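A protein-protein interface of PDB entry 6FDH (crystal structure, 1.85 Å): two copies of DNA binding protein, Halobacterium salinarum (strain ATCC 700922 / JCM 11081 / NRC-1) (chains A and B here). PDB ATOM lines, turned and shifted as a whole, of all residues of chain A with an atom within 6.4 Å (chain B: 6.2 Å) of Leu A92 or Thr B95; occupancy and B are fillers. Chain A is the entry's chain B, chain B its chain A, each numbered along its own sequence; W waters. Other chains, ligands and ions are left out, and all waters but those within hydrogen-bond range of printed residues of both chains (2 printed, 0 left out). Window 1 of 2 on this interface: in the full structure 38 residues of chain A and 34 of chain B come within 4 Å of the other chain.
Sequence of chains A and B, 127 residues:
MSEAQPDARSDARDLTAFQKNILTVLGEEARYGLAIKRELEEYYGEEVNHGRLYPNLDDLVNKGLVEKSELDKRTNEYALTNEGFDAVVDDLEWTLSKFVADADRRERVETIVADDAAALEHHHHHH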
ATOM      1  N   ASN A  21       6.926  -1.670 -16.746  1.00  0.00           N
ATOM      2  CA  ASN A  21       7.186  -2.656 -15.697  1.00  0.00           C
ATOM      3  C   ASN A  21       8.638  -3.125 -15.721  1.00  0.00           C
ATOM      4  O   ASN A  21       9.229  -3.383 -14.665  1.00  0.00           O
ATOM      5  CB  ASN A  21       6.222  -3.836 -15.841  1.00  0.00           C
ATOM      6  CG  ASN A  21       4.777  -3.471 -15.485  1.00  0.00           C
ATOM      7  OD1 ASN A  21       4.528  -2.507 -14.769  1.00  0.00           O
ATOM      8  ND2 ASN A  21       3.823  -4.255 -15.984  1.00  0.00           N
ATOM      9  N   THR A  24      10.445  -0.484 -13.963  1.00  0.00           N
ATOM     10  CA  THR A  24      10.215  -0.612 -12.525  1.00  0.00           C
ATOM     11  C   THR A  24      11.134  -1.673 -11.925  1.00  0.00           C
ATOM     12  O   THR A  24      11.754  -1.458 -10.876  1.00  0.00           O
ATOM     13  CB  THR A  24       8.753  -0.961 -12.253  1.00  0.00           C
ATOM     14  OG1 THR A  24       7.908   0.096 -12.732  1.00  0.00           O
ATOM     15  CG2 THR A  24       8.506  -1.145 -10.763  1.00  0.00           C
ATOM     16  N   ALA A  87      12.363   8.462 -15.906  1.00  0.00           N
ATOM     17  CA  ALA A  87      11.038   8.011 -16.326  1.00  0.00           C
ATOM     18  C   ALA A  87      10.316   7.267 -15.207  1.00  0.00           C
ATOM     19  O   ALA A  87       9.101   7.413 -15.050  1.00  0.00           O
ATOM     20  CB  ALA A  87      11.161   7.121 -17.563  1.00  0.00           C
ATOM     21  N   VAL A  88      11.045   6.459 -14.429  1.00  0.00           N
ATOM     22  CA  VAL A  88      10.454   5.771 -13.283  1.00  0.00           C
ATOM     23  C   VAL A  88       9.972   6.778 -12.236  1.00  0.00           C
ATOM     24  O   VAL A  88       8.848   6.680 -11.733  1.00  0.00           O
ATOM     25  CB  VAL A  88      11.469   4.773 -12.702  1.00  0.00           C
ATOM     26  CG1 VAL A  88      10.976   4.139 -11.403  1.00  0.00           C
ATOM     27  CG2 VAL A  88      11.780   3.712 -13.741  1.00  0.00           C
ATOM     28  N   VAL A  89      10.810   7.763 -11.889  1.00  0.00           N
ATOM     29  CA  VAL A  89      10.412   8.738 -10.874  1.00  0.00           C
ATOM     30  C   VAL A  89       9.245   9.589 -11.372  1.00  0.00           C
ATOM     31  O   VAL A  89       8.332   9.929 -10.612  1.00  0.00           O
ATOM     32  CB  VAL A  89      11.594   9.633 -10.452  1.00  0.00           C
ATOM     33  CG1 VAL A  89      12.699   8.830  -9.804  1.00  0.00           C
ATOM     34  CG2 VAL A  89      12.153  10.364 -11.617  1.00  0.00           C
ATOM     35  N   ASP A  90       9.279   9.973 -12.646  1.00  0.00           N
ATOM     36  CA  ASP A  90       8.230  10.814 -13.202  1.00  0.00           C
ATOM     37  C   ASP A  90       6.879  10.114 -13.152  1.00  0.00           C
ATOM     38  O   ASP A  90       5.866  10.729 -12.797  1.00  0.00           O
ATOM     39  CB  ASP A  90       8.587  11.187 -14.637  1.00  0.00           C
ATOM     40  CG  ASP A  90       7.446  11.829 -15.357  1.00  0.00           C
ATOM     41  OD1 ASP A  90       7.106  12.979 -14.993  1.00  0.00           O
ATOM     42  OD2 ASP A  90       6.873  11.175 -16.266  1.00  0.00           O
ATOM     43  N   ASP A  91       6.847   8.828 -13.505  1.00  0.00           N
ATOM     44  CA  ASP A  91       5.626   8.035 -13.373  1.00  0.00           C
ATOM     45  C   ASP A  91       5.191   7.933 -11.915  1.00  0.00           C
ATOM     46  O   ASP A  91       4.009   8.089 -11.595  1.00  0.00           O
ATOM     47  CB  ASP A  91       5.853   6.640 -13.977  1.00  0.00           C
ATOM     48  CG  ASP A  91       4.655   5.700 -13.793  1.00  0.00           C
ATOM     49  OD1 ASP A  91       3.676   5.836 -14.558  1.00  0.00           O
ATOM     50  OD2 ASP A  91       4.700   4.810 -12.898  1.00  0.00           O
ATOM     51  N   LEU A  92       6.133   7.669 -11.008  1.00  0.00           N
ATOM     52  CA  LEU A  92       5.775   7.552  -9.603  1.00  0.00           C
ATOM     53  C   LEU A  92       5.213   8.861  -9.076  1.00  0.00           C
ATOM     54  O   LEU A  92       4.223   8.864  -8.334  1.00  0.00           O
ATOM     55  CB  LEU A  92       6.989   7.125  -8.779  1.00  0.00           C
ATOM     56  CG  LEU A  92       6.761   6.988  -7.279  1.00  0.00           C
ATOM     57  CD1 LEU A  92       5.672   5.985  -6.980  1.00  0.00           C
ATOM     58  CD2 LEU A  92       8.057   6.569  -6.617  1.00  0.00           C
ATOM     59  N   GLU A  93       5.826   9.986  -9.453  1.00  0.00           N
ATOM     60  CA  GLU A  93       5.339  11.278  -8.992  1.00  0.00           C
ATOM     61  C   GLU A  93       3.928  11.537  -9.497  1.00  0.00           C
ATOM     62  O   GLU A  93       3.066  12.016  -8.746  1.00  0.00           O
ATOM     63  CB  GLU A  93       6.286  12.394  -9.442  1.00  0.00           C
ATOM     64  CG  GLU A  93       7.616  12.412  -8.681  1.00  0.00           C
ATOM     65  CD  GLU A  93       8.585  13.483  -9.156  1.00  0.00           C
ATOM     66  OE1 GLU A  93       8.364  14.102 -10.220  1.00  0.00           O
ATOM     67  OE2 GLU A  93       9.597  13.698  -8.459  1.00  0.00           O
ATOM     68  N   TRP A  94       3.665  11.233 -10.769  1.00  0.00           N
ATOM     69  CA  TRP A  94       2.319  11.437 -11.291  1.00  0.00           C
ATOM     70  C   TRP A  94       1.325  10.522 -10.584  1.00  0.00           C
ATOM     71  O   TRP A  94       0.265  10.963 -10.155  1.00  0.00           O
ATOM     72  CB  TRP A  94       2.274  11.222 -12.809  1.00  0.00           C
ATOM     73  CG  TRP A  94       0.914  11.580 -13.377  1.00  0.00           C
ATOM     74  CD1 TRP A  94       0.365  12.828 -13.496  1.00  0.00           C
ATOM     75  CD2 TRP A  94      -0.065  10.665 -13.877  1.00  0.00           C
ATOM     76  NE1 TRP A  94      -0.896  12.743 -14.036  1.00  0.00           N
ATOM     77  CE2 TRP A  94      -1.182  11.426 -14.284  1.00  0.00           C
ATOM     78  CE3 TRP A  94      -0.095   9.284 -14.036  1.00  0.00           C
ATOM     79  CZ2 TRP A  94      -2.317  10.844 -14.835  1.00  0.00           C
ATOM     80  CZ3 TRP A  94      -1.215   8.706 -14.569  1.00  0.00           C
ATOM     81  CH2 TRP A  94      -2.319   9.488 -14.972  1.00  0.00           C
ATOM     82  N   THR A  95       1.665   9.237 -10.432  1.00  0.00           N
ATOM     83  CA  THR A  95       0.799   8.322  -9.691  1.00  0.00           C
ATOM     84  C   THR A  95       0.522   8.837  -8.283  1.00  0.00           C
ATOM     85  O   THR A  95      -0.627   8.821  -7.814  1.00  0.00           O
ATOM     86  CB  THR A  95       1.452   6.934  -9.657  1.00  0.00           C
ATOM     87  OG1 THR A  95       1.278   6.328 -10.937  1.00  0.00           O
ATOM     88  CG2 THR A  95       0.862   6.040  -8.592  1.00  0.00           C
ATOM     89  N   LEU A  96       1.551   9.314  -7.595  1.00  0.00           N
ATOM     90  CA  LEU A  96       1.355   9.733  -6.216  1.00  0.00           C
ATOM     91  C   LEU A  96       0.583  11.043  -6.144  1.00  0.00           C
ATOM     92  O   LEU A  96      -0.183  11.265  -5.198  1.00  0.00           O
ATOM     93  CB  LEU A  96       2.709   9.860  -5.518  1.00  0.00           C
ATOM     94  CG  LEU A  96       3.426   8.538  -5.202  1.00  0.00           C
ATOM     95  CD1 LEU A  96       4.803   8.807  -4.645  1.00  0.00           C
ATOM     96  CD2 LEU A  96       2.616   7.747  -4.216  1.00  0.00           C
ATOM     97  N   SER A  97       0.776  11.923  -7.123  1.00  0.00           N
ATOM     98  CA  SER A  97       0.019  13.166  -7.142  1.00  0.00           C
ATOM     99  C   SER A  97      -1.480  12.916  -7.255  1.00  0.00           C
ATOM    100  O   SER A  97      -2.282  13.699  -6.736  1.00  0.00           O
ATOM    101  CB  SER A  97       0.483  14.034  -8.300  1.00  0.00           C
ATOM    102  OG  SER A  97      -0.408  15.117  -8.448  1.00  0.00           O
ATOM    103  N   ASP A 116       8.028  -1.071   3.623  1.00  0.00           N
ATOM    104  CA  ASP A 116       9.001  -1.506   2.625  1.00  0.00           C
ATOM    105  C   ASP A 116      10.415  -1.237   3.105  1.00  0.00           C
ATOM    106  O   ASP A 116      11.273  -2.127   3.076  1.00  0.00           O
ATOM    107  CB  ASP A 116       8.744  -0.808   1.290  1.00  0.00           C
ATOM    108  CG  ASP A 116       7.510  -1.327   0.598  1.00  0.00           C
ATOM    109  OD1 ASP A 116       6.975  -2.342   1.073  1.00  0.00           O
ATOM    110  OD2 ASP A 116       7.063  -0.718  -0.404  1.00  0.00           O
ATOM    111  N   ASP B  90      -2.935  -1.871  -5.754  1.00  0.00           N
ATOM    112  CA  ASP B  90      -2.067  -3.009  -6.029  1.00  0.00           C
ATOM    113  C   ASP B  90      -0.857  -2.596  -6.862  1.00  0.00           C
ATOM    114  O   ASP B  90       0.280  -2.959  -6.544  1.00  0.00           O
ATOM    115  CB  ASP B  90      -2.871  -4.104  -6.727  1.00  0.00           C
ATOM    116  CG  ASP B  90      -2.014  -5.266  -7.161  1.00  0.00           C
ATOM    117  OD1 ASP B  90      -1.486  -5.976  -6.276  1.00  0.00           O
ATOM    118  OD2 ASP B  90      -1.865  -5.472  -8.390  1.00  0.00           O
ATOM    119  N   ASP B  91      -1.072  -1.811  -7.922  1.00  0.00           N
ATOM    120  CA  ASP B  91       0.057  -1.411  -8.761  1.00  0.00           C
ATOM    121  C   ASP B  91       0.946  -0.396  -8.048  1.00  0.00           C
ATOM    122  O   ASP B  91       2.170  -0.432  -8.207  1.00  0.00           O
ATOM    123  CB  ASP B  91      -0.428  -0.842 -10.094  1.00  0.00           C
ATOM    124  CG  ASP B  91      -0.519  -1.898 -11.190  1.00  0.00           C
ATOM    125  OD1 ASP B  91      -0.132  -3.080 -10.974  1.00  0.00           O
ATOM    126  OD2 ASP B  91      -0.988  -1.542 -12.290  1.00  0.00           O
ATOM    127  N   LEU B  92       0.357   0.487  -7.240  1.00  0.00           N
ATOM    128  CA  LEU B  92       1.152   1.419  -6.453  1.00  0.00           C
ATOM    129  C   LEU B  92       2.038   0.691  -5.450  1.00  0.00           C
ATOM    130  O   LEU B  92       3.213   1.046  -5.279  1.00  0.00           O
ATOM    131  CB  LEU B  92       0.233   2.405  -5.733  1.00  0.00           C
ATOM    132  CG  LEU B  92       0.981   3.376  -4.819  1.00  0.00           C
ATOM    133  CD1 LEU B  92       2.011   4.188  -5.615  1.00  0.00           C
ATOM    134  CD2 LEU B  92       0.004   4.308  -4.136  1.00  0.00           C
ATOM    135  N   GLU B  93       1.493  -0.328  -4.775  1.00  0.00           N
ATOM    136  CA  GLU B  93       2.289  -1.132  -3.853  1.00  0.00           C
ATOM    137  C   GLU B  93       3.441  -1.818  -4.577  1.00  0.00           C
ATOM    138  O   GLU B  93       4.580  -1.840  -4.085  1.00  0.00           O
ATOM    139  CB  GLU B  93       1.404  -2.175  -3.165  1.00  0.00           C
ATOM    140  CG  GLU B  93       0.498  -1.593  -2.097  1.00  0.00           C
ATOM    141  CD  GLU B  93      -0.419  -2.613  -1.431  1.00  0.00           C
ATOM    142  OE1 GLU B  93      -0.463  -3.778  -1.880  1.00  0.00           O
ATOM    143  OE2 GLU B  93      -1.101  -2.241  -0.447  1.00  0.00           O
ATOM    144  N   TRP B  94       3.171  -2.418  -5.730  1.00  0.00           N
ATOM    145  CA  TRP B  94       4.242  -3.096  -6.447  1.00  0.00           C
ATOM    146  C   TRP B  94       5.319  -2.101  -6.868  1.00  0.00           C
ATOM    147  O   TRP B  94       6.513  -2.339  -6.679  1.00  0.00           O
ATOM    148  CB  TRP B  94       3.694  -3.861  -7.648  1.00  0.00           C
ATOM    149  CG  TRP B  94       4.756  -4.670  -8.339  1.00  0.00           C
ATOM    150  CD1 TRP B  94       5.333  -5.827  -7.895  1.00  0.00           C
ATOM    151  CD2 TRP B  94       5.366  -4.377  -9.594  1.00  0.00           C
ATOM    152  NE1 TRP B  94       6.269  -6.271  -8.801  1.00  0.00           N
ATOM    153  CE2 TRP B  94       6.306  -5.396  -9.853  1.00  0.00           C
ATOM    154  CE3 TRP B  94       5.202  -3.357 -10.529  1.00  0.00           C
ATOM    155  CZ2 TRP B  94       7.078  -5.417 -11.003  1.00  0.00           C
ATOM    156  CZ3 TRP B  94       5.959  -3.370 -11.647  1.00  0.00           C
ATOM    157  CH2 TRP B  94       6.896  -4.396 -11.889  1.00  0.00           C
ATOM    158  N   THR B  95       4.904  -0.972  -7.436  1.00  0.00           N
ATOM    159  CA  THR B  95       5.839   0.084  -7.813  1.00  0.00           C
ATOM    160  C   THR B  95       6.690   0.536  -6.629  1.00  0.00           C
ATOM    161  O   THR B  95       7.911   0.710  -6.754  1.00  0.00           O
ATOM    162  CB  THR B  95       5.036   1.250  -8.401  1.00  0.00           C
ATOM    163  OG1 THR B  95       4.443   0.830  -9.637  1.00  0.00           O
ATOM    164  CG2 THR B  95       5.903   2.445  -8.649  1.00  0.00           C
ATOM    165  N   LEU B  96       6.074   0.719  -5.465  1.00  0.00           N
ATOM    166  CA  LEU B  96       6.826   1.206  -4.313  1.00  0.00           C
ATOM    167  C   LEU B  96       7.733   0.123  -3.754  1.00  0.00           C
ATOM    168  O   LEU B  96       8.834   0.424  -3.276  1.00  0.00           O
ATOM    169  CB  LEU B  96       5.858   1.703  -3.241  1.00  0.00           C
ATOM    170  CG  LEU B  96       5.236   3.076  -3.518  1.00  0.00           C
ATOM    171  CD1 LEU B  96       4.125   3.338  -2.530  1.00  0.00           C
ATOM    172  CD2 LEU B  96       6.277   4.176  -3.456  1.00  0.00           C
ATOM    173  N   SER B  97       7.289  -1.135  -3.802  1.00  0.00           N
ATOM    174  CA  SER B  97       8.115  -2.238  -3.329  1.00  0.00           C
ATOM    175  C   SER B  97       9.414  -2.335  -4.115  1.00  0.00           C
ATOM    176  O   SER B  97      10.423  -2.812  -3.593  1.00  0.00           O
ATOM    177  CB  SER B  97       7.359  -3.561  -3.442  1.00  0.00           C
ATOM    178  OG  SER B  97       7.403  -4.071  -4.769  1.00  0.00           O
ATOM    179  N   LYS B  98       9.401  -1.908  -5.373  1.00  0.00           N
ATOM    180  CA  LYS B  98      10.601  -1.951  -6.193  1.00  0.00           C
ATOM    181  C   LYS B  98      11.391  -0.658  -6.133  1.00  0.00           C
ATOM    182  O   LYS B  98      12.619  -0.688  -6.271  1.00  0.00           O
ATOM    183  CB  LYS B  98      10.242  -2.256  -7.647  1.00  0.00           C
ATOM    184  CG  LYS B  98       9.592  -3.617  -7.861  1.00  0.00           C
ATOM    185  CD  LYS B  98      10.506  -4.741  -7.468  1.00  0.00           C
ATOM    186  CE  LYS B  98       9.833  -6.085  -7.658  1.00  0.00           C
ATOM    187  NZ  LYS B  98      10.557  -7.145  -6.908  1.00  0.00           N
ATOM    188  N   PHE B  99      10.721   0.469  -5.887  1.00  0.00           N
ATOM    189  CA  PHE B  99      11.402   1.757  -5.870  1.00  0.00           C
ATOM    190  C   PHE B  99      12.086   2.014  -4.537  1.00  0.00           C
ATOM    191  O   PHE B  99      13.177   2.586  -4.502  1.00  0.00           O
ATOM    192  CB  PHE B  99      10.426   2.898  -6.146  1.00  0.00           C
ATOM    193  CG  PHE B  99      11.103   4.229  -6.341  1.00  0.00           C
ATOM    194  CD1 PHE B  99      11.645   4.559  -7.562  1.00  0.00           C
ATOM    195  CD2 PHE B  99      11.202   5.143  -5.305  1.00  0.00           C
ATOM    196  CE1 PHE B  99      12.273   5.774  -7.757  1.00  0.00           C
ATOM    197  CE2 PHE B  99      11.822   6.358  -5.495  1.00  0.00           C
ATOM    198  CZ  PHE B  99      12.361   6.679  -6.722  1.00  0.00           C
ATOM    199  N   VAL B 100      11.459   1.598  -3.437  1.00  0.00           N
ATOM    200  CA  VAL B 100      11.967   1.890  -2.096  1.00  0.00           C
ATOM    201  C   VAL B 100      13.052   0.867  -1.803  1.00  0.00           C
ATOM    202  O   VAL B 100      12.841  -0.100  -1.063  1.00  0.00           O
ATOM    203  CB  VAL B 100      10.839   1.871  -1.048  1.00  0.00           C
ATOM    204  CG1 VAL B 100      11.370   2.145   0.360  1.00  0.00           C
ATOM    205  CG2 VAL B 100       9.789   2.909  -1.409  1.00  0.00           C
ATOM    206  N   VAL B 109      10.635   9.366  -1.620  1.00  0.00           N
ATOM    207  CA  VAL B 109       9.184   9.183  -1.665  1.00  0.00           C
ATOM    208  C   VAL B 109       8.506   9.944  -0.525  1.00  0.00           C
ATOM    209  O   VAL B 109       7.446  10.556  -0.711  1.00  0.00           O
ATOM    210  CB  VAL B 109       8.828   7.689  -1.623  1.00  0.00           C
ATOM    211  CG1 VAL B 109       7.320   7.516  -1.622  1.00  0.00           C
ATOM    212  CG2 VAL B 109       9.435   6.962  -2.812  1.00  0.00           C
ATOM    213  N   ILE B 112       8.153  13.436  -1.721  1.00  0.00           N
ATOM    214  CA  ILE B 112       7.110  13.567  -2.739  1.00  0.00           C
ATOM    215  C   ILE B 112       5.743  13.616  -2.081  1.00  0.00           C
ATOM    216  O   ILE B 112       4.929  14.507  -2.354  1.00  0.00           O
ATOM    217  CB  ILE B 112       7.185  12.408  -3.756  1.00  0.00           C
ATOM    218  CG1 ILE B 112       8.480  12.489  -4.563  1.00  0.00           C
ATOM    219  CG2 ILE B 112       5.944  12.429  -4.695  1.00  0.00           C
ATOM    220  CD1 ILE B 112       8.792  11.262  -5.366  1.00  0.00           C
HETATM  221  O   HOH W   1       4.994  -2.068  -1.288  1.00  0.00           O
HETATM  222  O   HOH W   2      11.716   0.736  -9.297  1.00  0.00           O
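The backbone NH of Ser B97 sits at hydrogen-bond distance from the side-chain carboxylate of Asp A116, at 3.4 Å.
Leu A92 touches Thr B95, and with the chains exchanged Thr A95 touches Leu B92.
Leu A96 touches Leu B92, but with the chains exchanged Leu A92 does not touch Leu B96 (4.01 Å).
8 positions are printed for both chains.
Water W1 lies within hydrogen-bond range of the side-chain carboxylate (OD2) of Asp A116 (2.6 Å) and the backbone carbonyl oxygen (O) of Glu B93 (2.8 Å).
Water W2 lies within hydrogen-bond range of O of Thr A24 (2.7 Å) and O of Lys B98 (3.5 Å).
Printed residues of chain B within 4 Å of Leu A92: Thr B95 and Phe B99.
Trp A94 touches none of the printed residues of chain B.
Of the printed residues of chain B, Asp A116 touches Leu B96 (3.5 Å) and Ser B97 (3.4 Å).
Asp B90 touches none of the printed residues of chain A.
Of the printed residues of chain A, Leu B96 touches Asp A116 (3.5 Å).
The nearest residue of chain A that does not touch Thr B95 is Thr A24 (4.2 Å).
The nearest printed residue of chain B that does not touch Asp A116 is Val B100 (4.1 Å).
O of Asp B91 is in hydrogen-bond range of OG1 of Thr B95.
The side-chain hydroxyl (OG) of Ser B97 lies within hydrogen-bond range of the backbone carbonyl oxygen (O) of Trp B94 (2.7 Å).
The backbone carbonyl oxygen (O) of Asp A91 lies within hydrogen-bond range of the side-chain hydroxyl (OG1) of Thr A95, 3.3 Å away.
OD1 of Asn A21 touches CZ3 of Trp B94 (3.5 Å).
Thr A24 touches Trp B94 (CG2 to CZ3, 3.5 Å).
Lys B98 touches Thr A24.
Phe B99 touches Val A88.
Phe B99 touches Val A89 (CE1 to CG1, 3.7 Å).
CD1 of Leu A92 touches CG2 of Thr B95, 3.9 Å away.
Phe B99 touches Leu A92.
Thr A95 touches Leu B92.
CD2 of Leu A96 touches CD1 of Leu B92, at 3.9 Å.
C of Leu B96 touches OD2 of Asp A116 (3.5 Å).
Of the 13 printed residues of chain B, 8 touch a printed residue of chain A.
Hydrophobic or aromatic side chains of chain B that line the printed part of chain A: Leu B92, Trp B94, Leu B96, Phe B99 and Ile B112.
Of the 14 printed residues of chain A, 9 touch a printed residue of chain B.
Hydrophobic or aromatic side chains of chain A within 4 Å of the printed part of chain B: Val A88, Val A89, Leu A92 and Leu A96.
Along chain A the printed residues that touch a printed residue of chain B span positions 21 to 116.
Among the printed residues, 13 pairs touch across the chains.
Among the printed residues, no Asp or Glu carboxylate lies within 4 Å of a Lys or Arg side-chain nitrogen of the other chain.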
